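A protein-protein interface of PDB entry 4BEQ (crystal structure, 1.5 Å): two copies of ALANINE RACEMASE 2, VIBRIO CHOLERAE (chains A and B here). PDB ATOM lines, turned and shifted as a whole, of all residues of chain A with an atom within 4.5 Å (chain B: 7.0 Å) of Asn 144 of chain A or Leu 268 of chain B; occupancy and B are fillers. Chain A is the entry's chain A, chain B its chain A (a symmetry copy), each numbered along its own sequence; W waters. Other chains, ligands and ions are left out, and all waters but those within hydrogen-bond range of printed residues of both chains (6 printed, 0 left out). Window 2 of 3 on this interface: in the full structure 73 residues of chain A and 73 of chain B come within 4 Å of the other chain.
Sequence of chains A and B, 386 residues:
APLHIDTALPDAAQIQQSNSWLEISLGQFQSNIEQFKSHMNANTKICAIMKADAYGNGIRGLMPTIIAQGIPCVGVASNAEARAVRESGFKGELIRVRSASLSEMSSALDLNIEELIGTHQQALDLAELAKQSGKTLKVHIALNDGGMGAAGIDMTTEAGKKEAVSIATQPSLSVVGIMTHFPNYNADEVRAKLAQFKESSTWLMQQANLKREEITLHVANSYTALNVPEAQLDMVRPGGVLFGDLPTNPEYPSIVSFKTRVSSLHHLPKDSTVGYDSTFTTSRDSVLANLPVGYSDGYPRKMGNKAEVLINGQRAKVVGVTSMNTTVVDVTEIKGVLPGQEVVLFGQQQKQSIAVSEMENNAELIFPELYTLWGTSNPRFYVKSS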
ATOM      1  N   ALA A 142      19.401   5.490  -3.279  1.00  0.00           N
ATOM      2  CA  ALA A 142      19.345   5.435  -1.834  1.00  0.00           C
ATOM      3  C   ALA A 142      19.612   6.824  -1.238  1.00  0.00           C
ATOM      4  O   ALA A 142      20.637   7.457  -1.540  1.00  0.00           O
ATOM      5  CB  ALA A 142      20.363   4.423  -1.312  1.00  0.00           C
ATOM      6  N   LEU A 143      18.694   7.275  -0.386  1.00  0.00           N
ATOM      7  CA  LEU A 143      18.824   8.544   0.312  1.00  0.00           C
ATOM      8  C   LEU A 143      19.135   8.286   1.782  1.00  0.00           C
ATOM      9  O   LEU A 143      18.818   7.201   2.306  1.00  0.00           O
ATOM     10  CB  LEU A 143      17.537   9.359   0.211  1.00  0.00           C
ATOM     11  CG  LEU A 143      16.963   9.611  -1.180  1.00  0.00           C
ATOM     12  CD1 LEU A 143      15.798  10.615  -1.087  1.00  0.00           C
ATOM     13  CD2 LEU A 143      17.989  10.140  -2.132  1.00  0.00           C
ATOM     14  N   ASN A 144      19.721   9.275   2.453  1.00  0.00           N
ATOM     15  CA  ASN A 144      20.099   9.136   3.853  1.00  0.00           C
ATOM     16  C   ASN A 144      19.127   9.741   4.885  1.00  0.00           C
ATOM     17  O   ASN A 144      19.511   9.952   6.021  1.00  0.00           O
ATOM     18  CB  ASN A 144      21.516   9.676   4.110  1.00  0.00           C
ATOM     19  CG  ASN A 144      22.113   9.132   5.396  1.00  0.00           C
ATOM     20  OD1 ASN A 144      21.971   7.934   5.715  1.00  0.00           O
ATOM     21  ND2 ASN A 144      22.742  10.008   6.172  1.00  0.00           N
ATOM     22  N   ASP A 145      17.877   9.984   4.511  1.00  0.00           N
ATOM     23  CA  ASP A 145      16.919  10.482   5.492  1.00  0.00           C
ATOM     24  C   ASP A 145      16.759   9.577   6.719  1.00  0.00           C
ATOM     25  O   ASP A 145      16.472  10.047   7.819  1.00  0.00           O
ATOM     26  CB  ASP A 145      15.579  10.755   4.823  1.00  0.00           C
ATOM     27  CG  ASP A 145      15.724  11.685   3.657  1.00  0.00           C
ATOM     28  OD1 ASP A 145      15.724  12.925   3.888  1.00  0.00           O
ATOM     29  OD2 ASP A 145      15.873  11.206   2.520  1.00  0.00           O
ATOM     30  N   GLY A 146      16.931   8.271   6.549  1.00  0.00           N
ATOM     31  CA  GLY A 146      16.888   7.368   7.683  1.00  0.00           C
ATOM     32  C   GLY A 146      18.054   7.501   8.650  1.00  0.00           C
ATOM     33  O   GLY A 146      17.957   7.095   9.813  1.00  0.00           O
ATOM     34  N   GLY A 147      19.185   8.022   8.172  1.00  0.00           N
ATOM     35  CA  GLY A 147      20.347   8.205   9.022  1.00  0.00           C
ATOM     36  C   GLY A 147      21.196   6.961   9.229  1.00  0.00           C
ATOM     37  O   GLY A 147      21.888   6.842  10.238  1.00  0.00           O
ATOM     38  N   MET A 148      21.170   6.040   8.271  1.00  0.00           N
ATOM     39  CA  MET A 148      22.066   4.888   8.337  1.00  0.00           C
ATOM     40  C   MET A 148      23.517   5.251   8.036  1.00  0.00           C
ATOM     41  O   MET A 148      24.437   4.551   8.459  1.00  0.00           O
ATOM     42  CB  MET A 148      21.607   3.781   7.383  1.00  0.00           C
ATOM     43  CG  MET A 148      20.462   2.952   7.904  1.00  0.00           C
ATOM     44  SD  MET A 148      20.875   1.887   9.307  1.00  0.00           S
ATOM     45  CE  MET A 148      21.766   0.566   8.491  1.00  0.00           C
ATOM     46  N   GLY A 149      23.727   6.324   7.284  1.00  0.00           N
ATOM     47  CA  GLY A 149      25.067   6.685   6.845  1.00  0.00           C
ATOM     48  C   GLY A 149      25.840   5.536   6.193  1.00  0.00           C
ATOM     49  O   GLY A 149      27.029   5.342   6.463  1.00  0.00           O
ATOM     50  N   GLY A 152      23.450   5.405   1.292  1.00  0.00           N
ATOM     51  CA  GLY A 152      22.695   6.487   0.683  1.00  0.00           C
ATOM     52  C   GLY A 152      23.449   7.783   0.482  1.00  0.00           C
ATOM     53  O   GLY A 152      24.561   7.970   0.951  1.00  0.00           O
ATOM     54  N   ILE A 153      22.824   8.680  -0.263  1.00  0.00           N
ATOM     55  CA  ILE A 153      23.354  10.014  -0.422  1.00  0.00           C
ATOM     56  C   ILE A 153      22.694  10.914   0.613  1.00  0.00           C
ATOM     57  O   ILE A 153      21.467  10.998   0.699  1.00  0.00           O
ATOM     58  CB  ILE A 153      23.144  10.548  -1.853  1.00  0.00           C
ATOM     59  CG1 ILE A 153      23.684  11.979  -1.965  1.00  0.00           C
ATOM     60  CG2 ILE A 153      21.672  10.531  -2.288  1.00  0.00           C
ATOM     61  CD1 ILE A 153      25.180  12.102  -1.685  1.00  0.00           C
ATOM     62  N   ASP A 154      23.530  11.558   1.411  1.00  0.00           N
ATOM     63  CA  ASP A 154      23.049  12.490   2.405  1.00  0.00           C
ATOM     64  C   ASP A 154      22.768  13.817   1.722  1.00  0.00           C
ATOM     65  O   ASP A 154      23.585  14.301   0.943  1.00  0.00           O
ATOM     66  CB  ASP A 154      24.071  12.657   3.515  1.00  0.00           C
ATOM     67  CG  ASP A 154      23.547  13.519   4.640  1.00  0.00           C
ATOM     68  OD1 ASP A 154      23.678  14.760   4.510  1.00  0.00           O
ATOM     69  OD2 ASP A 154      22.999  12.959   5.614  1.00  0.00           O
ATOM     70  N   THR A 180      14.902   4.892   1.404  1.00  0.00           N
ATOM     71  CA  THR A 180      15.794   5.035   2.532  1.00  0.00           C
ATOM     72  C   THR A 180      15.577   3.825   3.440  1.00  0.00           C
ATOM     73  O   THR A 180      14.801   2.931   3.115  1.00  0.00           O
ATOM     74  CB  THR A 180      15.639   6.413   3.278  1.00  0.00           C
ATOM     75  OG1 THR A 180      16.781   6.621   4.119  1.00  0.00           O
ATOM     76  CG2 THR A 180      14.374   6.484   4.099  1.00  0.00           C
ATOM     77  N   HIS B 266      31.333   7.677   0.523  1.00  0.00           N
ATOM     78  CA  HIS B 266      30.214   8.535   0.880  1.00  0.00           C
ATOM     79  C   HIS B 266      30.655   9.718   1.742  1.00  0.00           C
ATOM     80  O   HIS B 266      31.327   9.562   2.751  1.00  0.00           O
ATOM     81  CB  HIS B 266      29.181   7.718   1.647  1.00  0.00           C
ATOM     82  CG  HIS B 266      28.702   6.516   0.899  1.00  0.00           C
ATOM     83  ND1 HIS B 266      27.455   6.450   0.313  1.00  0.00           N
ATOM     84  CD2 HIS B 266      29.302   5.335   0.622  1.00  0.00           C
ATOM     85  CE1 HIS B 266      27.310   5.286  -0.285  1.00  0.00           C
ATOM     86  NE2 HIS B 266      28.425   4.591  -0.122  1.00  0.00           N
ATOM     87  N   HIS B 267      30.224  10.907   1.338  1.00  0.00           N
ATOM     88  CA  HIS B 267      30.483  12.113   2.100  1.00  0.00           C
ATOM     89  C   HIS B 267      29.359  12.322   3.107  1.00  0.00           C
ATOM     90  O   HIS B 267      28.185  12.414   2.726  1.00  0.00           O
ATOM     91  CB  HIS B 267      30.605  13.289   1.131  1.00  0.00           C
ATOM     92  CG  HIS B 267      31.832  13.220   0.279  1.00  0.00           C
ATOM     93  ND1 HIS B 267      31.977  12.309  -0.742  1.00  0.00           N
ATOM     94  CD2 HIS B 267      32.993  13.918   0.333  1.00  0.00           C
ATOM     95  CE1 HIS B 267      33.167  12.463  -1.300  1.00  0.00           C
ATOM     96  NE2 HIS B 267      33.801  13.430  -0.666  1.00  0.00           N
ATOM     97  N   LEU B 268      29.712  12.381   4.386  1.00  0.00           N
ATOM     98  CA  LEU B 268      28.728  12.499   5.450  1.00  0.00           C
ATOM     99  C   LEU B 268      29.137  13.627   6.393  1.00  0.00           C
ATOM    100  O   LEU B 268      30.239  13.618   6.919  1.00  0.00           O
ATOM    101  CB  LEU B 268      28.641  11.181   6.212  1.00  0.00           C
ATOM    102  CG  LEU B 268      27.416  11.018   7.096  1.00  0.00           C
ATOM    103  CD1 LEU B 268      26.150  10.948   6.250  1.00  0.00           C
ATOM    104  CD2 LEU B 268      27.557   9.775   7.961  1.00  0.00           C
ATOM    105  N   PRO B 269      28.262  14.623   6.574  1.00  0.00           N
ATOM    106  CA  PRO B 269      28.670  15.780   7.373  1.00  0.00           C
ATOM    107  C   PRO B 269      28.800  15.448   8.846  1.00  0.00           C
ATOM    108  O   PRO B 269      28.342  14.408   9.329  1.00  0.00           O
ATOM    109  CB  PRO B 269      27.530  16.791   7.151  1.00  0.00           C
ATOM    110  CG  PRO B 269      26.350  15.968   6.746  1.00  0.00           C
ATOM    111  CD  PRO B 269      26.901  14.761   6.027  1.00  0.00           C
ATOM    112  N   LYS B 270      29.456  16.348   9.565  1.00  0.00           N
ATOM    113  CA  LYS B 270      29.517  16.287  11.006  1.00  0.00           C
ATOM    114  C   LYS B 270      28.129  16.082  11.623  1.00  0.00           C
ATOM    115  O   LYS B 270      27.120  16.586  11.107  1.00  0.00           O
ATOM    116  CB  LYS B 270      30.144  17.590  11.520  1.00  0.00           C
ATOM    117  CG  LYS B 270      30.336  17.675  13.017  1.00  0.00           C
ATOM    118  CD  LYS B 270      30.855  19.062  13.391  1.00  0.00           C
ATOM    119  CE  LYS B 270      30.987  19.238  14.895  1.00  0.00           C
ATOM    120  NZ  LYS B 270      31.675  20.519  15.224  1.00  0.00           N
ATOM    121  N   ASP B 271      28.115  15.354  12.740  1.00  0.00           N
ATOM    122  CA  ASP B 271      26.909  15.070  13.527  1.00  0.00           C
ATOM    123  C   ASP B 271      25.896  14.162  12.810  1.00  0.00           C
ATOM    124  O   ASP B 271      24.681  14.298  12.973  1.00  0.00           O
ATOM    125  CB  ASP B 271      26.263  16.377  13.997  1.00  0.00           C
ATOM    126  CG  ASP B 271      27.204  17.215  14.869  1.00  0.00           C
ATOM    127  OD1 ASP B 271      27.973  16.636  15.671  1.00  0.00           O
ATOM    128  OD2 ASP B 271      27.177  18.458  14.745  1.00  0.00           O
ATOM    129  N   SER B 272      26.414  13.209  12.042  1.00  0.00           N
ATOM    130  CA  SER B 272      25.585  12.242  11.314  1.00  0.00           C
ATOM    131  C   SER B 272      25.732  10.855  11.920  1.00  0.00           C
ATOM    132  O   SER B 272      26.838  10.421  12.183  1.00  0.00           O
ATOM    133  CB  SER B 272      26.021  12.168   9.864  1.00  0.00           C
ATOM    134  OG  SER B 272      25.804  13.397   9.210  1.00  0.00           O
ATOM    135  N   THR B 273      24.619  10.165  12.125  1.00  0.00           N
ATOM    136  CA  THR B 273      24.632   8.813  12.690  1.00  0.00           C
ATOM    137  C   THR B 273      25.040   7.777  11.640  1.00  0.00           C
ATOM    138  O   THR B 273      24.839   7.973  10.446  1.00  0.00           O
ATOM    139  CB  THR B 273      23.250   8.447  13.256  1.00  0.00           C
ATOM    140  OG1 THR B 273      22.234   8.751  12.295  1.00  0.00           O
ATOM    141  CG2 THR B 273      22.984   9.258  14.531  1.00  0.00           C
ATOM    142  N   VAL B 274      25.645   6.691  12.111  1.00  0.00           N
ATOM    143  CA  VAL B 274      26.012   5.590  11.233  1.00  0.00           C
ATOM    144  C   VAL B 274      25.538   4.256  11.821  1.00  0.00           C
ATOM    145  O   VAL B 274      25.799   3.945  12.983  1.00  0.00           O
ATOM    146  CB  VAL B 274      27.539   5.540  11.009  1.00  0.00           C
ATOM    147  CG1 VAL B 274      27.885   4.414  10.036  1.00  0.00           C
ATOM    148  CG2 VAL B 274      28.064   6.873  10.516  1.00  0.00           C
ATOM    149  N   PHE B 280      27.220   5.186  16.462  1.00  0.00           N
ATOM    150  CA  PHE B 280      28.284   6.126  16.127  1.00  0.00           C
ATOM    151  C   PHE B 280      27.701   7.362  15.460  1.00  0.00           C
ATOM    152  O   PHE B 280      26.773   7.263  14.652  1.00  0.00           O
ATOM    153  CB  PHE B 280      29.292   5.451  15.175  1.00  0.00           C
ATOM    154  CG  PHE B 280      30.392   6.363  14.687  1.00  0.00           C
ATOM    155  CD1 PHE B 280      31.555   6.534  15.420  1.00  0.00           C
ATOM    156  CD2 PHE B 280      30.257   7.050  13.488  1.00  0.00           C
ATOM    157  CE1 PHE B 280      32.555   7.375  14.961  1.00  0.00           C
ATOM    158  CE2 PHE B 280      31.248   7.876  13.025  1.00  0.00           C
ATOM    159  CZ  PHE B 280      32.396   8.051  13.768  1.00  0.00           C
ATOM    160  N   THR B 282      29.319  10.959  13.568  1.00  0.00           N
ATOM    161  CA  THR B 282      30.515  11.654  13.106  1.00  0.00           C
ATOM    162  C   THR B 282      30.742  12.898  13.962  1.00  0.00           C
ATOM    163  O   THR B 282      29.786  13.551  14.394  1.00  0.00           O
ATOM    164  CB  THR B 282      30.403  12.080  11.630  1.00  0.00           C
ATOM    165  OG1 THR B 282      29.233  12.885  11.441  1.00  0.00           O
ATOM    166  CG2 THR B 282      30.307  10.863  10.708  1.00  0.00           C
ATOM    167  N   ARG B 284      32.923  15.181  12.697  1.00  0.00           N
ATOM    168  CA  ARG B 284      33.511  16.037  11.677  1.00  0.00           C
ATOM    169  C   ARG B 284      32.955  15.632  10.323  1.00  0.00           C
ATOM    170  O   ARG B 284      32.433  14.521  10.173  1.00  0.00           O
ATOM    171  CB  ARG B 284      35.029  15.849  11.645  1.00  0.00           C
ATOM    172  CG  ARG B 284      35.411  14.433  11.247  1.00  0.00           C
ATOM    173  CD  ARG B 284      36.895  14.161  11.301  1.00  0.00           C
ATOM    174  NE  ARG B 284      37.155  12.738  11.064  1.00  0.00           N
ATOM    175  CZ  ARG B 284      38.354  12.167  11.092  1.00  0.00           C
ATOM    176  NH1 ARG B 284      39.436  12.891  11.345  1.00  0.00           N
ATOM    177  NH2 ARG B 284      38.472  10.861  10.866  1.00  0.00           N
ATOM    178  N   ASP B 285      33.071  16.512   9.335  1.00  0.00           N
ATOM    179  CA  ASP B 285      32.737  16.137   7.966  1.00  0.00           C
ATOM    180  C   ASP B 285      33.631  14.949   7.591  1.00  0.00           C
ATOM    181  O   ASP B 285      34.853  14.968   7.775  1.00  0.00           O
ATOM    182  CB  ASP B 285      32.912  17.304   6.987  1.00  0.00           C
ATOM    183  CG  ASP B 285      31.820  18.378   7.130  1.00  0.00           C
ATOM    184  OD1 ASP B 285      30.875  18.201   7.929  1.00  0.00           O
ATOM    185  OD2 ASP B 285      31.910  19.405   6.420  1.00  0.00           O
ATOM    186  N   SER B 286      33.014  13.905   7.063  1.00  0.00           N
ATOM    187  CA  SER B 286      33.696  12.625   6.904  1.00  0.00           C
ATOM    188  C   SER B 286      33.581  12.070   5.484  1.00  0.00           C
ATOM    189  O   SER B 286      32.669  12.420   4.739  1.00  0.00           O
ATOM    190  CB  SER B 286      33.065  11.608   7.865  1.00  0.00           C
ATOM    191  OG  SER B 286      33.210  11.972   9.232  1.00  0.00           O
ATOM    192  N   VAL B 287      34.501  11.175   5.132  1.00  0.00           N
ATOM    193  CA  VAL B 287      34.332  10.326   3.956  1.00  0.00           C
ATOM    194  C   VAL B 287      34.352   8.890   4.472  1.00  0.00           C
ATOM    195  O   VAL B 287      35.302   8.468   5.153  1.00  0.00           O
ATOM    196  CB  VAL B 287      35.452  10.518   2.931  1.00  0.00           C
ATOM    197  CG1 VAL B 287      35.288   9.561   1.751  1.00  0.00           C
ATOM    198  CG2 VAL B 287      35.498  11.970   2.458  1.00  0.00           C
ATOM    199  N   LEU B 288      33.280   8.155   4.184  1.00  0.00           N
ATOM    200  CA  LEU B 288      33.118   6.797   4.690  1.00  0.00           C
ATOM    201  C   LEU B 288      33.153   5.825   3.532  1.00  0.00           C
ATOM    202  O   LEU B 288      32.534   6.059   2.480  1.00  0.00           O
ATOM    203  CB  LEU B 288      31.799   6.659   5.445  1.00  0.00           C
ATOM    204  CG  LEU B 288      31.607   7.653   6.598  1.00  0.00           C
ATOM    205  CD1 LEU B 288      30.264   7.395   7.278  1.00  0.00           C
ATOM    206  CD2 LEU B 288      32.745   7.554   7.599  1.00  0.00           C
ATOM    207  N   THR B 332      38.323   9.226   6.204  1.00  0.00           N
ATOM    208  CA  THR B 332      38.442  10.677   6.130  1.00  0.00           C
ATOM    209  C   THR B 332      39.902  11.121   6.023  1.00  0.00           C
ATOM    210  O   THR B 332      40.228  12.008   5.234  1.00  0.00           O
ATOM    211  CB  THR B 332      37.810  11.330   7.348  1.00  0.00           C
ATOM    212  OG1 THR B 332      36.413  11.003   7.407  1.00  0.00           O
ATOM    213  CG2 THR B 332      37.954  12.848   7.274  1.00  0.00           C
HETATM  214  O   HOH W   1      27.002   9.265  -0.576  1.00  0.00           O
HETATM  215  O   HOH W   2      22.255   5.386  12.494  1.00  0.00           O
HETATM  216  O   HOH W   3      26.867  14.364   1.168  1.00  0.00           O
HETATM  217  O   HOH W   4      26.280  10.603   1.808  1.00  0.00           O
HETATM  218  O   HOH W   5      23.424   9.703   8.837  1.00  0.00           O
HETATM  219  O   HOH W   6      23.418  13.883   8.223  1.00  0.00           O
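O of Gly 147 of chain A lies within hydrogen-bond range of OG1 of Thr 273 of chain B (2.8 Å). A ring nitrogen (ND1) of His 266 of chain B sits at hydrogen-bond distance from the backbone carbonyl oxygen (O) of Gly 152 of chain A (3.3 Å).
The backbone NH (N) of Met 148 of chain A sits at hydrogen-bond distance from the side-chain amide oxygen (OD1) of Asn 144 of chain A (3.3 Å). The backbone NH (N) of Asn 144 of chain A is in hydrogen-bond range of the backbone carbonyl oxygen (O) of Ile 153 of chain A (3.0 Å). The side-chain amide nitrogen of Asn 144 of chain A sits at hydrogen-bond distance from the side-chain carboxylate of Asp 154 of chain A, at 3.0 Å. The backbone NH (N) of Ser 286 of chain B sits at hydrogen-bond distance from the backbone carbonyl oxygen (O) of Leu 268 of chain B, 2.8 Å away. O of Pro 269 of chain B lies within hydrogen-bond range of OG of Ser 272 of chain B (2.7 Å). The backbone carbonyl oxygen of Pro 269 of chain B sits at hydrogen-bond distance from the side-chain hydroxyl of Thr 282 of chain B.
Among the printed residues, merely in contact across the chains: Met 148 of chain A with Val 274 of chain B, Asn 144 of chain A with Leu 268 of chain B, Asp 154 of chain A with Pro 269 of chain B, Gly 149 of chain A with Thr 273 of chain B, Gly 149 of chain A with Val 274 of chain B, Asp 154 of chain A with Leu 268 of chain B, Met 148 of chain A with Thr 273 of chain B and Gly 149 of chain A with Leu 288 of chain B.
Asn 144 of chain A touches just one residue of chain B: Leu 268 (3.5 Å). Leu 268 of chain B touches two residues of chain A. Of the printed residues of chain A, His 266 of chain B touches Gly 152. Of the printed residues of chain B, Gly 147 of chain A touches Thr 273 (2.8 Å).
Of the 12 printed residues of chain A, 6 touch a printed residue of chain B. Hydrophobic or aromatic side chains of chain B within 4 Å of the printed part of chain A: His 266, Leu 268, Pro 269, Val 274 and Leu 288. Among the printed residues, 10 pairs touch across the chains. Among the printed residues, no Asp or Glu carboxylate lies within 4 Å of a Lys or Arg side-chain nitrogen of the other chain.
No position is printed for both chains.
Water W6 bridges OG of Ser 272 of chain B (2.6 Å) and OD2 of Asp 154 of chain A (2.8 Å). Water W2 lies within hydrogen-bond range of the backbone carbonyl oxygen (O) of Gly 147 of chain A and the side-chain hydroxyl (OG1) of Thr 273 of chain B. Water W5 bridges O of Thr 273 of chain B (2.8 Å) and ND2 of Asn 144 of chain A (2.8 Å). Water W4 lies within hydrogen-bond range of O of His 267 of chain B (2.8 Å), N of Asp 154 of chain A (2.9 Å) and O of Gly 152 of chain A (3.3 Å). Water W3 lies within hydrogen-bond range of the backbone carbonyl oxygen of His 267 of chain B and the backbone carbonyl oxygen of Asp 154 of chain A. Water W1 lies within hydrogen-bond range of a ring nitrogen (ND1) of His 266 of chain B (3.0 Å) and the backbone carbonyl oxygen (O) of Gly 152 of chain A (3.2 Å).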
